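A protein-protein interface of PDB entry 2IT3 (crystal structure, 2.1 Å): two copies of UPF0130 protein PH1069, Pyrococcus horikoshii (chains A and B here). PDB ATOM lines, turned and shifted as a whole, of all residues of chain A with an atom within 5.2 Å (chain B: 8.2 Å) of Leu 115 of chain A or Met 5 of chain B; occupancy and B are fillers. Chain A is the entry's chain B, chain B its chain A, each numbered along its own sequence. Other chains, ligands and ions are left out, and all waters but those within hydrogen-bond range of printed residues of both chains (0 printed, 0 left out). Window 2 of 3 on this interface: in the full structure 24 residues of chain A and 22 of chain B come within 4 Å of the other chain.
Of chain B, only Met 5 (3.5 Å) and Ile 138 (3.7 Å) come within 4 Å of Leu 115 of chain A.
Of the printed residues of chain B, Ile 135 of chain A touches Ile 135 (3.0 Å).
Printed residues of chain B within 4 Å of Ile 138 of chain A: Leu 115 and Ile 135.
Met 5 of chain B touches just one residue of chain A: Leu 115.
Of the printed residues of chain A, Leu 115 of chain B touches Ile 138.
Of the printed residues of chain A, Ile 135 of chain B touches Ile 135 (3.0 Å) and Ile 138 (3.7 Å).
The nearest residue of chain B that does not touch Leu 115 of chain A is Leu 115 of chain B (4.1 Å).
Leu 115 of chain A touches Ile 138 of chain B, and with the chains exchanged Ile 138 of chain A touches Leu 115 of chain B.
Ile 135 of chain B touches its own counterpart, Ile 135 of chain A.
Ile 138 of chain A touches Ile 135 of chain B, but with the chains exchanged Ile 135 of chain A does not touch Ile 138 of chain B (4.1 Å).
Positions printed for both chains: 7, 113, 114, 115, 116, 135, 138 and 143.
Leu 115 of chain A touches Met 5 of chain B (CD2 to SD, 3.5 Å).
CD1 of Leu 115 of chain A touches CD1 of Ile 138 of chain B, 3.7 Å away.
Val 119 of chain A touches Ile 138 of chain B (CG2 to CB, 3.8 Å).
Leu 115 of chain B touches Ile 138 of chain A (CD1 to CD1, 3.6 Å).
Ile 138 of chain A touches Ile 135 of chain B.
N of Ile 135 of chain A lies within hydrogen-bond range of O of Ile 135 of chain B (3.0 Å).
The side-chain hydroxyl of Thr 8 of chain B sits close to the backbone carbonyl oxygen of Met 5 of chain B (3.4 Å).
Hydrophobic or aromatic side chains of chain B that line the printed part of chain A: Met 5, Leu 115, Ile 135 and Ile 138.
Of the 11 printed residues of chain A, 4 touch a printed residue of chain B.
Among the printed residues, no Asp or Glu carboxylate lies within 4 Å of a Lys or Arg side-chain nitrogen of the other chain.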
ATOM      1  N   PHE A   7       1.484 -14.155   0.676  1.00  0.00           N
ATOM      2  CA  PHE A   7       1.294 -12.980  -0.168  1.00  0.00           C
ATOM      3  C   PHE A   7       1.555 -11.726   0.659  1.00  0.00           C
ATOM      4  O   PHE A   7       1.925 -10.685   0.118  1.00  0.00           O
ATOM      5  CB  PHE A   7      -0.129 -12.954  -0.745  1.00  0.00           C
ATOM      6  CG  PHE A   7      -1.203 -12.767   0.289  1.00  0.00           C
ATOM      7  CD1 PHE A   7      -1.551 -11.496   0.733  1.00  0.00           C
ATOM      8  CD2 PHE A   7      -1.854 -13.863   0.834  1.00  0.00           C
ATOM      9  CE1 PHE A   7      -2.528 -11.328   1.702  1.00  0.00           C
ATOM     10  CE2 PHE A   7      -2.831 -13.701   1.804  1.00  0.00           C
ATOM     11  CZ  PHE A   7      -3.166 -12.435   2.238  1.00  0.00           C
ATOM     12  N   LYS A 113      -2.492  -6.222   0.501  1.00  0.00           N
ATOM     13  CA  LYS A 113      -1.532  -6.643   1.514  1.00  0.00           C
ATOM     14  C   LYS A 113      -2.050  -7.779   2.379  1.00  0.00           C
ATOM     15  O   LYS A 113      -1.419  -8.826   2.483  1.00  0.00           O
ATOM     16  CB  LYS A 113      -1.189  -5.452   2.406  1.00  0.00           C
ATOM     17  CG  LYS A 113      -0.337  -5.778   3.620  1.00  0.00           C
ATOM     18  CD  LYS A 113       1.144  -5.732   3.306  1.00  0.00           C
ATOM     19  CE  LYS A 113       1.879  -4.925   4.366  1.00  0.00           C
ATOM     20  NZ  LYS A 113       1.310  -3.540   4.462  1.00  0.00           N
ATOM     21  N   THR A 114      -3.196  -7.553   3.010  1.00  0.00           N
ATOM     22  CA  THR A 114      -3.807  -8.549   3.871  1.00  0.00           C
ATOM     23  C   THR A 114      -5.225  -8.873   3.409  1.00  0.00           C
ATOM     24  O   THR A 114      -5.850  -8.113   2.658  1.00  0.00           O
ATOM     25  CB  THR A 114      -3.893  -8.056   5.327  1.00  0.00           C
ATOM     26  OG1 THR A 114      -4.889  -7.030   5.421  1.00  0.00           O
ATOM     27  CG2 THR A 114      -2.540  -7.496   5.788  1.00  0.00           C
ATOM     28  N   LEU A 115      -5.727 -10.009   3.873  1.00  0.00           N
ATOM     29  CA  LEU A 115      -7.068 -10.440   3.531  1.00  0.00           C
ATOM     30  C   LEU A 115      -8.040  -9.329   3.917  1.00  0.00           C
ATOM     31  O   LEU A 115      -8.968  -9.027   3.180  1.00  0.00           O
ATOM     32  CB  LEU A 115      -7.402 -11.726   4.290  1.00  0.00           C
ATOM     33  CG  LEU A 115      -8.629 -12.524   3.852  1.00  0.00           C
ATOM     34  CD1 LEU A 115      -8.494 -12.911   2.374  1.00  0.00           C
ATOM     35  CD2 LEU A 115      -8.756 -13.771   4.729  1.00  0.00           C
ATOM     36  N   GLU A 116      -7.798  -8.711   5.070  1.00  0.00           N
ATOM     37  CA  GLU A 116      -8.640  -7.629   5.575  1.00  0.00           C
ATOM     38  C   GLU A 116      -8.724  -6.432   4.621  1.00  0.00           C
ATOM     39  O   GLU A 116      -9.784  -5.837   4.469  1.00  0.00           O
ATOM     40  CB  GLU A 116      -8.110  -7.162   6.929  1.00  0.00           C
ATOM     41  CG  GLU A 116      -8.931  -6.086   7.608  1.00  0.00           C
ATOM     42  CD  GLU A 116      -8.196  -5.478   8.795  1.00  0.00           C
ATOM     43  OE1 GLU A 116      -7.666  -6.249   9.624  1.00  0.00           O
ATOM     44  OE2 GLU A 116      -8.145  -4.233   8.901  1.00  0.00           O
ATOM     45  N   ASP A 117      -7.609  -6.065   3.994  1.00  0.00           N
ATOM     46  CA  ASP A 117      -7.612  -4.942   3.059  1.00  0.00           C
ATOM     47  C   ASP A 117      -8.484  -5.280   1.852  1.00  0.00           C
ATOM     48  O   ASP A 117      -9.209  -4.428   1.331  1.00  0.00           O
ATOM     49  CB  ASP A 117      -6.190  -4.626   2.587  1.00  0.00           C
ATOM     50  CG  ASP A 117      -5.274  -4.213   3.723  1.00  0.00           C
ATOM     51  OD1 ASP A 117      -5.650  -3.279   4.470  1.00  0.00           O
ATOM     52  OD2 ASP A 117      -4.184  -4.821   3.863  1.00  0.00           O
ATOM     53  N   ALA A 118      -8.403  -6.534   1.420  1.00  0.00           N
ATOM     54  CA  ALA A 118      -9.169  -7.021   0.276  1.00  0.00           C
ATOM     55  C   ALA A 118     -10.672  -6.888   0.493  1.00  0.00           C
ATOM     56  O   ALA A 118     -11.398  -6.419  -0.389  1.00  0.00           O
ATOM     57  CB  ALA A 118      -8.815  -8.468   0.005  1.00  0.00           C
ATOM     58  N   VAL A 119     -11.134  -7.306   1.668  1.00  0.00           N
ATOM     59  CA  VAL A 119     -12.552  -7.230   2.012  1.00  0.00           C
ATOM     60  C   VAL A 119     -13.032  -5.786   2.036  1.00  0.00           C
ATOM     61  O   VAL A 119     -14.134  -5.478   1.594  1.00  0.00           O
ATOM     62  CB  VAL A 119     -12.825  -7.864   3.397  1.00  0.00           C
ATOM     63  CG1 VAL A 119     -14.254  -7.537   3.866  1.00  0.00           C
ATOM     64  CG2 VAL A 119     -12.622  -9.371   3.314  1.00  0.00           C
ATOM     65  N   ILE A 135     -12.722 -11.431  -4.642  1.00  0.00           N
ATOM     66  CA  ILE A 135     -11.330 -11.834  -4.514  1.00  0.00           C
ATOM     67  C   ILE A 135     -11.155 -12.868  -5.608  1.00  0.00           C
ATOM     68  O   ILE A 135     -11.702 -13.969  -5.528  1.00  0.00           O
ATOM     69  CB  ILE A 135     -11.044 -12.459  -3.125  1.00  0.00           C
ATOM     70  CG1 ILE A 135     -11.170 -11.369  -2.050  1.00  0.00           C
ATOM     71  CG2 ILE A 135      -9.668 -13.107  -3.113  1.00  0.00           C
ATOM     72  CD1 ILE A 135     -10.847 -11.809  -0.636  1.00  0.00           C
ATOM     73  N   ILE A 138      -6.032 -16.101  -4.515  1.00  0.00           N
ATOM     74  CA  ILE A 138      -5.157 -16.026  -3.367  1.00  0.00           C
ATOM     75  C   ILE A 138      -4.089 -17.064  -3.644  1.00  0.00           C
ATOM     76  O   ILE A 138      -4.403 -18.229  -3.887  1.00  0.00           O
ATOM     77  CB  ILE A 138      -5.875 -16.401  -2.065  1.00  0.00           C
ATOM     78  CG1 ILE A 138      -7.081 -15.488  -1.850  1.00  0.00           C
ATOM     79  CG2 ILE A 138      -4.902 -16.284  -0.894  1.00  0.00           C
ATOM     80  CD1 ILE A 138      -7.857 -15.811  -0.607  1.00  0.00           C
ATOM     81  N   LEU A 143      -2.561 -11.648  -3.476  1.00  0.00           N
ATOM     82  CA  LEU A 143      -4.003 -11.754  -3.297  1.00  0.00           C
ATOM     83  C   LEU A 143      -4.616 -10.690  -4.208  1.00  0.00           C
ATOM     84  O   LEU A 143      -4.421  -9.492  -3.997  1.00  0.00           O
ATOM     85  CB  LEU A 143      -4.376 -11.485  -1.839  1.00  0.00           C
ATOM     86  CG  LEU A 143      -5.844 -11.653  -1.421  1.00  0.00           C
ATOM     87  CD1 LEU A 143      -5.940 -11.592   0.095  1.00  0.00           C
ATOM     88  CD2 LEU A 143      -6.704 -10.573  -2.051  1.00  0.00           C
ATOM     89  N   TYR B   4      -5.812 -18.460  11.775  1.00  0.00           N
ATOM     90  CA  TYR B   4      -7.201 -18.827  12.184  1.00  0.00           C
ATOM     91  C   TYR B   4      -8.116 -17.612  12.056  1.00  0.00           C
ATOM     92  O   TYR B   4      -7.681 -16.474  12.271  1.00  0.00           O
ATOM     93  CB  TYR B   4      -7.212 -19.318  13.633  1.00  0.00           C
ATOM     94  CG  TYR B   4      -8.421 -20.148  13.995  1.00  0.00           C
ATOM     95  CD1 TYR B   4      -8.734 -21.304  13.280  1.00  0.00           C
ATOM     96  CD2 TYR B   4      -9.236 -19.800  15.071  1.00  0.00           C
ATOM     97  CE1 TYR B   4      -9.828 -22.095  13.627  1.00  0.00           C
ATOM     98  CE2 TYR B   4     -10.337 -20.587  15.427  1.00  0.00           C
ATOM     99  CZ  TYR B   4     -10.625 -21.731  14.700  1.00  0.00           C
ATOM    100  OH  TYR B   4     -11.712 -22.508  15.033  1.00  0.00           O
ATOM    101  N   MET B   5      -9.380 -17.850  11.711  1.00  0.00           N
ATOM    102  CA  MET B   5     -10.334 -16.758  11.557  1.00  0.00           C
ATOM    103  C   MET B   5     -11.766 -17.075  11.949  1.00  0.00           C
ATOM    104  O   MET B   5     -12.210 -18.218  11.861  1.00  0.00           O
ATOM    105  CB  MET B   5     -10.309 -16.251  10.127  1.00  0.00           C
ATOM    106  CG  MET B   5      -9.004 -15.612   9.757  1.00  0.00           C
ATOM    107  SD  MET B   5      -9.092 -15.041   7.965  1.00  0.00           S
ATOM    108  CE  MET B   5      -8.598 -16.690   7.087  1.00  0.00           C
ATOM    109  N   ARG B   6     -12.483 -16.030  12.354  1.00  0.00           N
ATOM    110  CA  ARG B   6     -13.868 -16.130  12.802  1.00  0.00           C
ATOM    111  C   ARG B   6     -14.838 -16.964  11.961  1.00  0.00           C
ATOM    112  O   ARG B   6     -15.711 -17.640  12.515  1.00  0.00           O
ATOM    113  CB  ARG B   6     -14.433 -14.723  13.013  1.00  0.00           C
ATOM    114  CG  ARG B   6     -14.763 -14.415  14.472  1.00  0.00           C
ATOM    115  CD  ARG B   6     -14.703 -12.925  14.774  1.00  0.00           C
ATOM    116  NE  ARG B   6     -13.338 -12.409  14.671  1.00  0.00           N
ATOM    117  CZ  ARG B   6     -12.968 -11.183  15.031  1.00  0.00           C
ATOM    118  NH1 ARG B   6     -13.860 -10.331  15.522  1.00  0.00           N
ATOM    119  NH2 ARG B   6     -11.702 -10.806  14.899  1.00  0.00           N
ATOM    120  N   PHE B   7     -14.714 -16.934  10.639  1.00  0.00           N
ATOM    121  CA  PHE B   7     -15.633 -17.729   9.842  1.00  0.00           C
ATOM    122  C   PHE B   7     -15.329 -19.222  10.027  1.00  0.00           C
ATOM    123  O   PHE B   7     -16.202 -20.072   9.862  1.00  0.00           O
ATOM    124  CB  PHE B   7     -15.589 -17.303   8.362  1.00  0.00           C
ATOM    125  CG  PHE B   7     -14.313 -17.636   7.653  1.00  0.00           C
ATOM    126  CD1 PHE B   7     -14.107 -18.899   7.118  1.00  0.00           C
ATOM    127  CD2 PHE B   7     -13.324 -16.676   7.491  1.00  0.00           C
ATOM    128  CE1 PHE B   7     -12.936 -19.204   6.430  1.00  0.00           C
ATOM    129  CE2 PHE B   7     -12.152 -16.969   6.809  1.00  0.00           C
ATOM    130  CZ  PHE B   7     -11.958 -18.237   6.275  1.00  0.00           C
ATOM    131  N   THR B   8     -14.092 -19.535  10.397  1.00  0.00           N
ATOM    132  CA  THR B   8     -13.711 -20.920  10.631  1.00  0.00           C
ATOM    133  C   THR B   8     -14.342 -21.343  11.960  1.00  0.00           C
ATOM    134  O   THR B   8     -14.931 -22.417  12.081  1.00  0.00           O
ATOM    135  CB  THR B   8     -12.179 -21.063  10.715  1.00  0.00           C
ATOM    136  OG1 THR B   8     -11.587 -20.552   9.514  1.00  0.00           O
ATOM    137  CG2 THR B   8     -11.784 -22.527  10.883  1.00  0.00           C
ATOM    138  N   GLU B   9     -14.228 -20.464  12.949  1.00  0.00           N
ATOM    139  CA  GLU B   9     -14.772 -20.688  14.281  1.00  0.00           C
ATOM    140  C   GLU B   9     -16.283 -20.892  14.180  1.00  0.00           C
ATOM    141  O   GLU B   9     -16.863 -21.708  14.902  1.00  0.00           O
ATOM    142  CB  GLU B   9     -14.468 -19.462  15.156  1.00  0.00           C
ATOM    143  CG  GLU B   9     -14.311 -19.707  16.661  1.00  0.00           C
ATOM    144  CD  GLU B   9     -15.598 -20.121  17.345  1.00  0.00           C
ATOM    145  OE1 GLU B   9     -15.892 -21.339  17.390  1.00  0.00           O
ATOM    146  OE2 GLU B   9     -16.321 -19.225  17.834  1.00  0.00           O
ATOM    147  N   ASN B  10     -16.913 -20.166  13.260  1.00  0.00           N
ATOM    148  CA  ASN B  10     -18.363 -20.236  13.091  1.00  0.00           C
ATOM    149  C   ASN B  10     -18.863 -21.228  12.044  1.00  0.00           C
ATOM    150  O   ASN B  10     -20.073 -21.415  11.889  1.00  0.00           O
ATOM    151  CB  ASN B  10     -18.898 -18.843  12.757  1.00  0.00           C
ATOM    152  CG  ASN B  10     -20.400 -18.790  12.740  1.00  0.00           C
ATOM    153  OD1 ASN B  10     -21.051 -19.110  13.730  1.00  0.00           O
ATOM    154  ND2 ASN B  10     -20.965 -18.382  11.613  1.00  0.00           N
ATOM    155  N   PHE B  11     -17.942 -21.868  11.336  1.00  0.00           N
ATOM    156  CA  PHE B  11     -18.315 -22.817  10.293  1.00  0.00           C
ATOM    157  C   PHE B  11     -19.313 -23.882  10.742  1.00  0.00           C
ATOM    158  O   PHE B  11     -20.314 -24.136  10.070  1.00  0.00           O
ATOM    159  CB  PHE B  11     -17.075 -23.510   9.739  1.00  0.00           C
ATOM    160  CG  PHE B  11     -17.373 -24.435   8.598  1.00  0.00           C
ATOM    161  CD1 PHE B  11     -17.609 -23.932   7.325  1.00  0.00           C
ATOM    162  CD2 PHE B  11     -17.458 -25.807   8.804  1.00  0.00           C
ATOM    163  CE1 PHE B  11     -17.927 -24.783   6.274  1.00  0.00           C
ATOM    164  CE2 PHE B  11     -17.777 -26.667   7.757  1.00  0.00           C
ATOM    165  CZ  PHE B  11     -18.011 -26.154   6.490  1.00  0.00           C
ATOM    166  N   LYS B 113     -14.894 -23.810   5.007  1.00  0.00           N
ATOM    167  CA  LYS B 113     -14.413 -23.822   6.379  1.00  0.00           C
ATOM    168  C   LYS B 113     -13.145 -22.991   6.573  1.00  0.00           C
ATOM    169  O   LYS B 113     -12.995 -22.318   7.595  1.00  0.00           O
ATOM    170  CB  LYS B 113     -14.171 -25.270   6.813  1.00  0.00           C
ATOM    171  CG  LYS B 113     -13.581 -25.449   8.207  1.00  0.00           C
ATOM    172  CD  LYS B 113     -13.076 -26.884   8.356  1.00  0.00           C
ATOM    173  CE  LYS B 113     -12.247 -27.092   9.608  1.00  0.00           C
ATOM    174  NZ  LYS B 113     -11.551 -28.423   9.571  1.00  0.00           N
ATOM    175  N   THR B 114     -12.234 -23.047   5.604  1.00  0.00           N
ATOM    176  CA  THR B 114     -10.992 -22.288   5.670  1.00  0.00           C
ATOM    177  C   THR B 114     -10.650 -21.670   4.324  1.00  0.00           C
ATOM    178  O   THR B 114     -11.272 -21.973   3.304  1.00  0.00           O
ATOM    179  CB  THR B 114      -9.785 -23.162   6.075  1.00  0.00           C
ATOM    180  OG1 THR B 114      -9.536 -24.134   5.050  1.00  0.00           O
ATOM    181  CG2 THR B 114     -10.045 -23.861   7.407  1.00  0.00           C
ATOM    182  N   LEU B 115      -9.636 -20.817   4.331  1.00  0.00           N
ATOM    183  CA  LEU B 115      -9.176 -20.140   3.128  1.00  0.00           C
ATOM    184  C   LEU B 115      -8.648 -21.185   2.152  1.00  0.00           C
ATOM    185  O   LEU B 115      -8.849 -21.095   0.941  1.00  0.00           O
ATOM    186  CB  LEU B 115      -8.071 -19.151   3.505  1.00  0.00           C
ATOM    187  CG  LEU B 115      -7.863 -17.932   2.607  1.00  0.00           C
ATOM    188  CD1 LEU B 115      -9.177 -17.191   2.438  1.00  0.00           C
ATOM    189  CD2 LEU B 115      -6.811 -17.027   3.222  1.00  0.00           C
ATOM    190  N   GLU B 116      -7.976 -22.186   2.706  1.00  0.00           N
ATOM    191  CA  GLU B 116      -7.393 -23.282   1.945  1.00  0.00           C
ATOM    192  C   GLU B 116      -8.483 -24.047   1.189  1.00  0.00           C
ATOM    193  O   GLU B 116      -8.322 -24.389   0.016  1.00  0.00           O
ATOM    194  CB  GLU B 116      -6.670 -24.219   2.918  1.00  0.00           C
ATOM    195  CG  GLU B 116      -5.751 -25.251   2.291  1.00  0.00           C
ATOM    196  CD  GLU B 116      -5.249 -26.259   3.315  1.00  0.00           C
ATOM    197  OE1 GLU B 116      -4.763 -25.833   4.390  1.00  0.00           O
ATOM    198  OE2 GLU B 116      -5.340 -27.479   3.048  1.00  0.00           O
ATOM    199  N   ILE B 135     -13.990 -15.912  -4.726  1.00  0.00           N
ATOM    200  CA  ILE B 135     -14.396 -15.750  -3.340  1.00  0.00           C
ATOM    201  C   ILE B 135     -15.219 -14.455  -3.328  1.00  0.00           C
ATOM    202  O   ILE B 135     -14.689 -13.363  -3.538  1.00  0.00           O
ATOM    203  CB  ILE B 135     -13.166 -15.643  -2.419  1.00  0.00           C
ATOM    204  CG1 ILE B 135     -12.518 -17.021  -2.287  1.00  0.00           C
ATOM    205  CG2 ILE B 135     -13.564 -15.140  -1.047  1.00  0.00           C
ATOM    206  CD1 ILE B 135     -11.261 -17.031  -1.444  1.00  0.00           C
ATOM    207  N   ILE B 138     -16.264 -12.383   2.653  1.00  0.00           N
ATOM    208  CA  ILE B 138     -15.686 -12.879   3.892  1.00  0.00           C
ATOM    209  C   ILE B 138     -16.158 -12.044   5.076  1.00  0.00           C
ATOM    210  O   ILE B 138     -15.875 -10.859   5.190  1.00  0.00           O
ATOM    211  CB  ILE B 138     -14.156 -12.796   3.813  1.00  0.00           C
ATOM    212  CG1 ILE B 138     -13.594 -13.839   2.841  1.00  0.00           C
ATOM    213  CG2 ILE B 138     -13.556 -13.079   5.200  1.00  0.00           C
ATOM    214  CD1 ILE B 138     -12.064 -13.788   2.777  1.00  0.00           C
ATOM    215  N   SER B 139     -16.948 -12.691   5.943  1.00  0.00           N
ATOM    216  CA  SER B 139     -17.364 -12.031   7.170  1.00  0.00           C
ATOM    217  C   SER B 139     -16.851 -12.798   8.381  1.00  0.00           C
ATOM    218  O   SER B 139     -16.108 -13.763   8.266  1.00  0.00           O
ATOM    219  CB  SER B 139     -18.890 -11.991   7.185  1.00  0.00           C
ATOM    220  OG  SER B 139     -19.387 -13.325   7.103  1.00  0.00           O
ATOM    221  N   ASN B 140     -17.220 -12.302   9.576  1.00  0.00           N
ATOM    222  CA  ASN B 140     -16.882 -13.060  10.765  1.00  0.00           C
ATOM    223  C   ASN B 140     -17.827 -14.250  10.957  1.00  0.00           C
ATOM    224  O   ASN B 140     -17.811 -14.931  11.970  1.00  0.00           O
ATOM    225  CB  ASN B 140     -16.941 -12.123  11.977  1.00  0.00           C
ATOM    226  CG  ASN B 140     -18.374 -11.817  12.331  1.00  0.00           C
ATOM    227  OD1 ASN B 140     -18.785 -10.663  12.445  1.00  0.00           O
ATOM    228  ND2 ASN B 140     -19.152 -12.894  12.524  1.00  0.00           N
ATOM    229  N   LYS B 141     -18.700 -14.474   9.948  1.00  0.00           N
ATOM    230  CA  LYS B 141     -19.635 -15.594  10.039  1.00  0.00           C
ATOM    231  C   LYS B 141     -19.347 -16.679   8.985  1.00  0.00           C
ATOM    232  O   LYS B 141     -19.414 -17.868   9.254  1.00  0.00           O
ATOM    233  CB  LYS B 141     -21.059 -15.058   9.839  1.00  0.00           C
ATOM    234  CG  LYS B 141     -21.396 -13.908  10.791  1.00  0.00           C
ATOM    235  CD  LYS B 141     -22.784 -13.326  10.511  1.00  0.00           C
ATOM    236  CE  LYS B 141     -23.044 -12.033  11.291  1.00  0.00           C
ATOM    237  NZ  LYS B 141     -24.343 -11.481  10.911  1.00  0.00           N
ATOM    238  N   LEU B 143     -17.504 -17.667   4.757  1.00  0.00           N
ATOM    239  CA  LEU B 143     -16.744 -17.368   3.558  1.00  0.00           C
ATOM    240  C   LEU B 143     -17.537 -17.997   2.426  1.00  0.00           C
ATOM    241  O   LEU B 143     -17.729 -19.209   2.394  1.00  0.00           O
ATOM    242  CB  LEU B 143     -15.341 -17.979   3.625  1.00  0.00           C
ATOM    243  CG  LEU B 143     -14.416 -17.566   2.474  1.00  0.00           C
ATOM    244  CD1 LEU B 143     -12.962 -17.762   2.873  1.00  0.00           C
ATOM    245  CD2 LEU B 143     -14.753 -18.369   1.230  1.00  0.00           C
